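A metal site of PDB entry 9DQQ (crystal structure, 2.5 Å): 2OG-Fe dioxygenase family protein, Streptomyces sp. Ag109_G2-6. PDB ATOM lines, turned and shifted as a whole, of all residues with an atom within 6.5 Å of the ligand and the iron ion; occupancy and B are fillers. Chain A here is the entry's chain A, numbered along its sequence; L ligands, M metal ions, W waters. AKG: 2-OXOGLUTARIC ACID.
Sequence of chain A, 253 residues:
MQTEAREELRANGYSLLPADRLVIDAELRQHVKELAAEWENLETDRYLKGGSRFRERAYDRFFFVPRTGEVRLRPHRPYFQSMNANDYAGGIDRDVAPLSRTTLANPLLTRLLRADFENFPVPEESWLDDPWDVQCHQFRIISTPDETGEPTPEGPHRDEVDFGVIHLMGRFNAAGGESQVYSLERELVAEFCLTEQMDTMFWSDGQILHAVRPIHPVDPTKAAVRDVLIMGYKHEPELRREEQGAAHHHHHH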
ATOM      1  N   ARG A  55      24.090  -9.901  29.134  1.00  0.00           N
ATOM      2  CA  ARG A  55      25.054 -10.490  28.214  1.00  0.00           C
ATOM      3  C   ARG A  55      25.812 -11.595  28.945  1.00  0.00           C
ATOM      4  O   ARG A  55      26.528 -11.320  29.904  1.00  0.00           O
ATOM      5  CB  ARG A  55      26.022  -9.444  27.662  1.00  0.00           C
ATOM      6  CG  ARG A  55      27.278 -10.049  27.045  1.00  0.00           C
ATOM      7  CD  ARG A  55      28.022  -9.069  26.137  1.00  0.00           C
ATOM      8  NE  ARG A  55      27.569  -9.170  24.750  1.00  0.00           N
ATOM      9  CZ  ARG A  55      28.226  -8.670  23.703  1.00  0.00           C
ATOM     10  NH1 ARG A  55      29.371  -8.009  23.849  1.00  0.00           N
ATOM     11  NH2 ARG A  55      27.723  -8.822  22.478  1.00  0.00           N
ATOM     12  N   PHE A 139      28.679 -15.784  22.832  1.00  0.00           N
ATOM     13  CA  PHE A 139      27.872 -14.648  23.278  1.00  0.00           C
ATOM     14  C   PHE A 139      26.414 -15.050  23.312  1.00  0.00           C
ATOM     15  O   PHE A 139      25.886 -15.542  22.305  1.00  0.00           O
ATOM     16  CB  PHE A 139      27.984 -13.421  22.360  1.00  0.00           C
ATOM     17  CG  PHE A 139      29.184 -12.598  22.589  1.00  0.00           C
ATOM     18  CD1 PHE A 139      29.492 -12.141  23.860  1.00  0.00           C
ATOM     19  CD2 PHE A 139      30.024 -12.268  21.523  1.00  0.00           C
ATOM     20  CE1 PHE A 139      30.614 -11.371  24.073  1.00  0.00           C
ATOM     21  CE2 PHE A 139      31.168 -11.500  21.741  1.00  0.00           C
ATOM     22  CZ  PHE A 139      31.456 -11.049  23.013  1.00  0.00           C
ATOM     23  N   ILE A 141      22.955 -12.937  23.969  1.00  0.00           N
ATOM     24  CA  ILE A 141      22.328 -11.641  24.179  1.00  0.00           C
ATOM     25  C   ILE A 141      20.897 -11.853  24.653  1.00  0.00           C
ATOM     26  O   ILE A 141      20.119 -12.536  23.978  1.00  0.00           O
ATOM     27  CB  ILE A 141      22.351 -10.789  22.901  1.00  0.00           C
ATOM     28  CG1 ILE A 141      23.758 -10.741  22.327  1.00  0.00           C
ATOM     29  CG2 ILE A 141      21.878  -9.375  23.207  1.00  0.00           C
ATOM     30  CD1 ILE A 141      24.728 -10.034  23.232  1.00  0.00           C
ATOM     31  N   GLU A 154      26.081  -1.170  20.784  1.00  0.00           N
ATOM     32  CA  GLU A 154      27.416  -0.726  20.401  1.00  0.00           C
ATOM     33  C   GLU A 154      27.416  -0.296  18.943  1.00  0.00           C
ATOM     34  O   GLU A 154      26.781  -0.926  18.098  1.00  0.00           O
ATOM     35  CB  GLU A 154      28.478  -1.818  20.627  1.00  0.00           C
ATOM     36  CG  GLU A 154      29.878  -1.350  20.228  1.00  0.00           C
ATOM     37  CD  GLU A 154      30.974  -2.344  20.565  1.00  0.00           C
ATOM     38  OE1 GLU A 154      30.676  -3.402  21.157  1.00  0.00           O
ATOM     39  OE2 GLU A 154      32.149  -2.049  20.219  1.00  0.00           O
ATOM     40  N   HIS A 157      32.319  -0.696  14.561  1.00  0.00           N
ATOM     41  CA  HIS A 157      33.641  -0.987  15.108  1.00  0.00           C
ATOM     42  C   HIS A 157      34.295  -2.087  14.285  1.00  0.00           C
ATOM     43  O   HIS A 157      33.669  -2.712  13.426  1.00  0.00           O
ATOM     44  CB  HIS A 157      33.543  -1.406  16.576  1.00  0.00           C
ATOM     45  CG  HIS A 157      32.873  -2.719  16.792  1.00  0.00           C
ATOM     46  ND1 HIS A 157      31.502  -2.884  16.751  1.00  0.00           N
ATOM     47  CD2 HIS A 157      33.389  -3.944  17.053  1.00  0.00           C
ATOM     48  CE1 HIS A 157      31.208  -4.151  16.983  1.00  0.00           C
ATOM     49  NE2 HIS A 157      32.336  -4.816  17.171  1.00  0.00           N
ATOM     50  N   ARG A 158      35.582  -2.305  14.551  1.00  0.00           N
ATOM     51  CA  ARG A 158      36.290  -3.496  14.098  1.00  0.00           C
ATOM     52  C   ARG A 158      36.684  -4.306  15.318  1.00  0.00           C
ATOM     53  O   ARG A 158      36.693  -3.794  16.444  1.00  0.00           O
ATOM     54  CB  ARG A 158      37.538  -3.123  13.305  1.00  0.00           C
ATOM     55  CG  ARG A 158      38.606  -2.464  14.152  1.00  0.00           C
ATOM     56  CD  ARG A 158      39.854  -2.280  13.353  1.00  0.00           C
ATOM     57  NE  ARG A 158      40.289  -3.549  12.791  1.00  0.00           N
ATOM     58  CZ  ARG A 158      41.454  -3.725  12.177  1.00  0.00           C
ATOM     59  NH1 ARG A 158      42.323  -2.745  12.047  1.00  0.00           N
ATOM     60  NH2 ARG A 158      41.751  -4.921  11.673  1.00  0.00           N
ATOM     61  N   ASP A 159      36.988  -5.582  15.117  1.00  0.00           N
ATOM     62  CA  ASP A 159      37.364  -6.380  16.276  1.00  0.00           C
ATOM     63  C   ASP A 159      38.862  -6.377  16.541  1.00  0.00           C
ATOM     64  O   ASP A 159      39.288  -6.966  17.539  1.00  0.00           O
ATOM     65  CB  ASP A 159      36.829  -7.818  16.161  1.00  0.00           C
ATOM     66  CG  ASP A 159      35.321  -7.870  16.299  1.00  0.00           C
ATOM     67  OD1 ASP A 159      34.714  -6.813  16.580  1.00  0.00           O
ATOM     68  OD2 ASP A 159      34.715  -8.945  16.127  1.00  0.00           O
ATOM     69  N   ILE A 166      31.266 -15.285  12.255  1.00  0.00           N
ATOM     70  CA  ILE A 166      30.193 -15.343  13.222  1.00  0.00           C
ATOM     71  C   ILE A 166      29.213 -16.380  12.729  1.00  0.00           C
ATOM     72  O   ILE A 166      28.826 -16.368  11.560  1.00  0.00           O
ATOM     73  CB  ILE A 166      29.516 -13.960  13.449  1.00  0.00           C
ATOM     74  CG1 ILE A 166      28.262 -14.118  14.302  1.00  0.00           C
ATOM     75  CG2 ILE A 166      29.163 -13.280  12.142  1.00  0.00           C
ATOM     76  CD1 ILE A 166      27.706 -12.814  14.779  1.00  0.00           C
ATOM     77  N   GLY A 177      18.108  -7.336  15.530  1.00  0.00           N
ATOM     78  CA  GLY A 177      19.393  -8.027  15.471  1.00  0.00           C
ATOM     79  C   GLY A 177      19.984  -8.125  14.087  1.00  0.00           C
ATOM     80  O   GLY A 177      20.606  -9.137  13.753  1.00  0.00           O
ATOM     81  N   GLU A 178      19.805  -7.088  13.282  1.00  0.00           N
ATOM     82  CA  GLU A 178      20.389  -7.031  11.949  1.00  0.00           C
ATOM     83  C   GLU A 178      21.874  -6.696  12.054  1.00  0.00           C
ATOM     84  O   GLU A 178      22.261  -5.810  12.821  1.00  0.00           O
ATOM     85  CB  GLU A 178      19.683  -5.972  11.100  1.00  0.00           C
ATOM     86  CG  GLU A 178      18.230  -6.272  10.768  1.00  0.00           C
ATOM     87  CD  GLU A 178      17.250  -5.895  11.881  1.00  0.00           C
ATOM     88  OE1 GLU A 178      17.672  -5.484  12.985  1.00  0.00           O
ATOM     89  OE2 GLU A 178      16.040  -5.999  11.620  1.00  0.00           O
ATOM     90  N   SER A 179      22.719  -7.383  11.303  1.00  0.00           N
ATOM     91  CA  SER A 179      24.151  -7.119  11.324  1.00  0.00           C
ATOM     92  C   SER A 179      24.443  -6.033  10.292  1.00  0.00           C
ATOM     93  O   SER A 179      24.001  -6.139   9.132  1.00  0.00           O
ATOM     94  CB  SER A 179      24.973  -8.378  11.002  1.00  0.00           C
ATOM     95  OG  SER A 179      24.441  -9.524  11.609  1.00  0.00           O
ATOM     96  N   LEU A 194      21.209 -12.830  10.172  1.00  0.00           N
ATOM     97  CA  LEU A 194      21.361 -14.205  10.615  1.00  0.00           C
ATOM     98  C   LEU A 194      20.070 -14.620  11.306  1.00  0.00           C
ATOM     99  O   LEU A 194      19.733 -14.089  12.364  1.00  0.00           O
ATOM    100  CB  LEU A 194      22.579 -14.331  11.531  1.00  0.00           C
ATOM    101  CG  LEU A 194      23.838 -13.690  10.911  1.00  0.00           C
ATOM    102  CD1 LEU A 194      25.005 -13.850  11.841  1.00  0.00           C
ATOM    103  CD2 LEU A 194      24.159 -14.298   9.571  1.00  0.00           C
ATOM    104  N   MET A 201      28.632 -15.619   8.694  1.00  0.00           N
ATOM    105  CA  MET A 201      29.148 -14.433   8.044  1.00  0.00           C
ATOM    106  C   MET A 201      30.644 -14.332   8.301  1.00  0.00           C
ATOM    107  O   MET A 201      31.064 -14.348   9.467  1.00  0.00           O
ATOM    108  CB  MET A 201      28.450 -13.175   8.563  1.00  0.00           C
ATOM    109  CG  MET A 201      28.785 -11.973   7.730  1.00  0.00           C
ATOM    110  SD  MET A 201      30.036 -10.957   8.476  1.00  0.00           S
ATOM    111  CE  MET A 201      29.209 -10.428   9.970  1.00  0.00           C
ATOM    112  N   TRP A 203      34.212 -11.995   7.579  1.00  0.00           N
ATOM    113  CA  TRP A 203      34.575 -10.636   7.210  1.00  0.00           C
ATOM    114  C   TRP A 203      36.070 -10.387   7.352  1.00  0.00           C
ATOM    115  O   TRP A 203      36.760 -10.995   8.181  1.00  0.00           O
ATOM    116  CB  TRP A 203      33.784  -9.600   8.014  1.00  0.00           C
ATOM    117  CG  TRP A 203      34.273  -9.288   9.421  1.00  0.00           C
ATOM    118  CD1 TRP A 203      35.077  -8.244   9.801  1.00  0.00           C
ATOM    119  CD2 TRP A 203      33.919  -9.981  10.636  1.00  0.00           C
ATOM    120  NE1 TRP A 203      35.246  -8.242  11.177  1.00  0.00           N
ATOM    121  CE2 TRP A 203      34.562  -9.319  11.707  1.00  0.00           C
ATOM    122  CE3 TRP A 203      33.121 -11.091  10.920  1.00  0.00           C
ATOM    123  CZ2 TRP A 203      34.447  -9.734  13.034  1.00  0.00           C
ATOM    124  CZ3 TRP A 203      33.010 -11.520  12.245  1.00  0.00           C
ATOM    125  CH2 TRP A 203      33.651 -10.824  13.292  1.00  0.00           C
ATOM    126  N   ASP A 205      38.526  -7.853   8.769  1.00  0.00           N
ATOM    127  CA  ASP A 205      38.299  -6.924   9.867  1.00  0.00           C
ATOM    128  C   ASP A 205      39.010  -5.572   9.682  1.00  0.00           C
ATOM    129  O   ASP A 205      38.702  -4.631  10.423  1.00  0.00           O
ATOM    130  CB  ASP A 205      38.720  -7.584  11.184  1.00  0.00           C
ATOM    131  CG  ASP A 205      38.302  -6.764  12.384  1.00  0.00           C
ATOM    132  OD1 ASP A 205      37.084  -6.658  12.641  1.00  0.00           O
ATOM    133  OD2 ASP A 205      39.184  -6.230  13.072  1.00  0.00           O
ATOM    134  N   HIS A 210      31.807  -2.832  11.470  1.00  0.00           N
ATOM    135  CA  HIS A 210      30.620  -3.650  11.636  1.00  0.00           C
ATOM    136  C   HIS A 210      29.943  -3.304  12.941  1.00  0.00           C
ATOM    137  O   HIS A 210      30.501  -2.603  13.795  1.00  0.00           O
ATOM    138  CB  HIS A 210      30.968  -5.139  11.530  1.00  0.00           C
ATOM    139  CG  HIS A 210      31.733  -5.677  12.707  1.00  0.00           C
ATOM    140  ND1 HIS A 210      33.104  -5.834  12.687  1.00  0.00           N
ATOM    141  CD2 HIS A 210      31.325  -6.081  13.932  1.00  0.00           C
ATOM    142  CE1 HIS A 210      33.501  -6.317  13.853  1.00  0.00           C
ATOM    143  NE2 HIS A 210      32.446  -6.479  14.624  1.00  0.00           N
ATOM    144  N   ALA A 211      28.724  -3.806  13.090  1.00  0.00           N
ATOM    145  CA  ALA A 211      27.863  -3.560  14.232  1.00  0.00           C
ATOM    146  C   ALA A 211      26.670  -4.488  14.103  1.00  0.00           C
ATOM    147  O   ALA A 211      26.408  -5.025  13.032  1.00  0.00           O
ATOM    148  CB  ALA A 211      27.417  -2.097  14.299  1.00  0.00           C
ATOM    149  N   VAL A 212      25.948  -4.663  15.195  1.00  0.00           N
ATOM    150  CA  VAL A 212      24.695  -5.400  15.155  1.00  0.00           C
ATOM    151  C   VAL A 212      23.622  -4.575  15.853  1.00  0.00           C
ATOM    152  O   VAL A 212      23.880  -3.934  16.875  1.00  0.00           O
ATOM    153  CB  VAL A 212      24.823  -6.809  15.790  1.00  0.00           C
ATOM    154  CG1 VAL A 212      25.087  -6.729  17.291  1.00  0.00           C
ATOM    155  CG2 VAL A 212      23.550  -7.605  15.529  1.00  0.00           C
ATOM    156  N   ARG A 226      19.447 -14.239  21.615  1.00  0.00           N
ATOM    157  CA  ARG A 226      20.227 -14.439  20.401  1.00  0.00           C
ATOM    158  C   ARG A 226      21.604 -15.010  20.745  1.00  0.00           C
ATOM    159  O   ARG A 226      22.380 -14.347  21.446  1.00  0.00           O
ATOM    160  CB  ARG A 226      20.364 -13.110  19.639  1.00  0.00           C
ATOM    161  CG  ARG A 226      21.200 -13.138  18.365  1.00  0.00           C
ATOM    162  CD  ARG A 226      21.132 -11.796  17.616  1.00  0.00           C
ATOM    163  NE  ARG A 226      21.725 -11.864  16.286  1.00  0.00           N
ATOM    164  CZ  ARG A 226      22.979 -11.510  16.012  1.00  0.00           C
ATOM    165  NH1 ARG A 226      23.792 -11.057  16.953  1.00  0.00           N
ATOM    166  NH2 ARG A 226      23.425 -11.602  14.756  1.00  0.00           N
ATOM    167  N   VAL A 228      25.273 -16.406  19.469  1.00  0.00           N
ATOM    168  CA  VAL A 228      26.224 -16.348  18.355  1.00  0.00           C
ATOM    169  C   VAL A 228      27.592 -16.850  18.810  1.00  0.00           C
ATOM    170  O   VAL A 228      28.011 -16.613  19.947  1.00  0.00           O
ATOM    171  CB  VAL A 228      26.326 -14.931  17.759  1.00  0.00           C
ATOM    172  CG1 VAL A 228      24.942 -14.446  17.289  1.00  0.00           C
ATOM    173  CG2 VAL A 228      26.957 -13.957  18.746  1.00  0.00           C
ATOM    174  N   ILE A 230      31.486 -16.372  17.766  1.00  0.00           N
ATOM    175  CA  ILE A 230      32.317 -15.444  17.023  1.00  0.00           C
ATOM    176  C   ILE A 230      33.768 -15.885  17.143  1.00  0.00           C
ATOM    177  O   ILE A 230      34.240 -16.154  18.261  1.00  0.00           O
ATOM    178  CB  ILE A 230      32.175 -13.989  17.501  1.00  0.00           C
ATOM    179  CG1 ILE A 230      30.729 -13.528  17.405  1.00  0.00           C
ATOM    180  CG2 ILE A 230      33.090 -13.039  16.660  1.00  0.00           C
ATOM    181  CD1 ILE A 230      30.569 -11.994  17.565  1.00  0.00           C
HETATM  182  C1  AKG L   1      30.545  -8.249  19.125  1.00  0.00           C
HETATM  183  O1  AKG L   1      29.914  -8.810  20.046  1.00  0.00           O
HETATM  184  O2  AKG L   1      31.732  -7.863  19.062  1.00  0.00           O
HETATM  185  C2  AKG L   1      29.723  -7.996  17.827  1.00  0.00           C
HETATM  186  O5  AKG L   1      30.196  -7.309  16.923  1.00  0.00           O
HETATM  187  C3  AKG L   1      28.363  -8.636  17.761  1.00  0.00           C
HETATM  188  C4  AKG L   1      28.043  -9.194  16.397  1.00  0.00           C
HETATM  189  C5  AKG L   1      26.706  -9.934  16.344  1.00  0.00           C
HETATM  190  O3  AKG L   1      26.087  -9.976  15.266  1.00  0.00           O
HETATM  191  O4  AKG L   1      26.368 -10.436  17.441  1.00  0.00           O
HETATM  192 FE    FE M   1      32.561  -6.932  16.664  1.00  0.00          FE
HETATM  193  O   HOH W   1      31.980  -8.860  16.017  1.00  0.00           O
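An oxygen (O4) of the ligand lies within salt-bridge range of the guanidinium group of Arg 226 (2.7 Å).
The guanidinium group (NH2) of Arg 55 is in salt-bridge range of an oxygen (O1) of the ligand, at 3.3 Å.
N of Ile 166 sits at hydrogen-bond distance from O of Met 201, at 2.9 Å.
N of Asp 159 sits at hydrogen-bond distance from OD1 of Asp 205, 2.7 Å away.
N of Val 228 lies within hydrogen-bond range of O of Phe 139, 3.0 Å away.
O of Arg 226 is in hydrogen-bond range of N of Ile 141, 2.9 Å away.
Merely in contact with the ligand: Ile 166 (3.3 Å), Phe 139 (3.4 Å), Val 212 (3.4 Å), Val 228 (3.8 Å) and Ile 230 (3.9 Å).
Within 4 Å of the ligand: Arg 55, Phe 139, His 157, Ile 166, His 210, Val 212, Arg 226, Val 228 and Ile 230.
The nearest printed residue that does not touch the ligand is Asp 159 (4.02 Å).
Three residues have an atom within 4 Å of the iron ion: His 157, Asp 159 and His 210.
The iron ion is bound by a ring nitrogen (NE2) of His 210 (2.1 Å).
The iron ion is bound by water W1, at 2.1 Å.
OD1 of Asp 159 is bound to the iron ion, 2.2 Å away.
The iron ion is bound by NE2 of His 157 (2.2 Å).
An oxygen (O5) of the ligand is bound to the iron ion.
Slightly farther from the iron ion lies an oxygen (O2) of the ligand (2.7 Å).
Water W1 bridges OD2 of Asp 159 (2.7 Å) and O2 of the ligand (3.2 Å).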
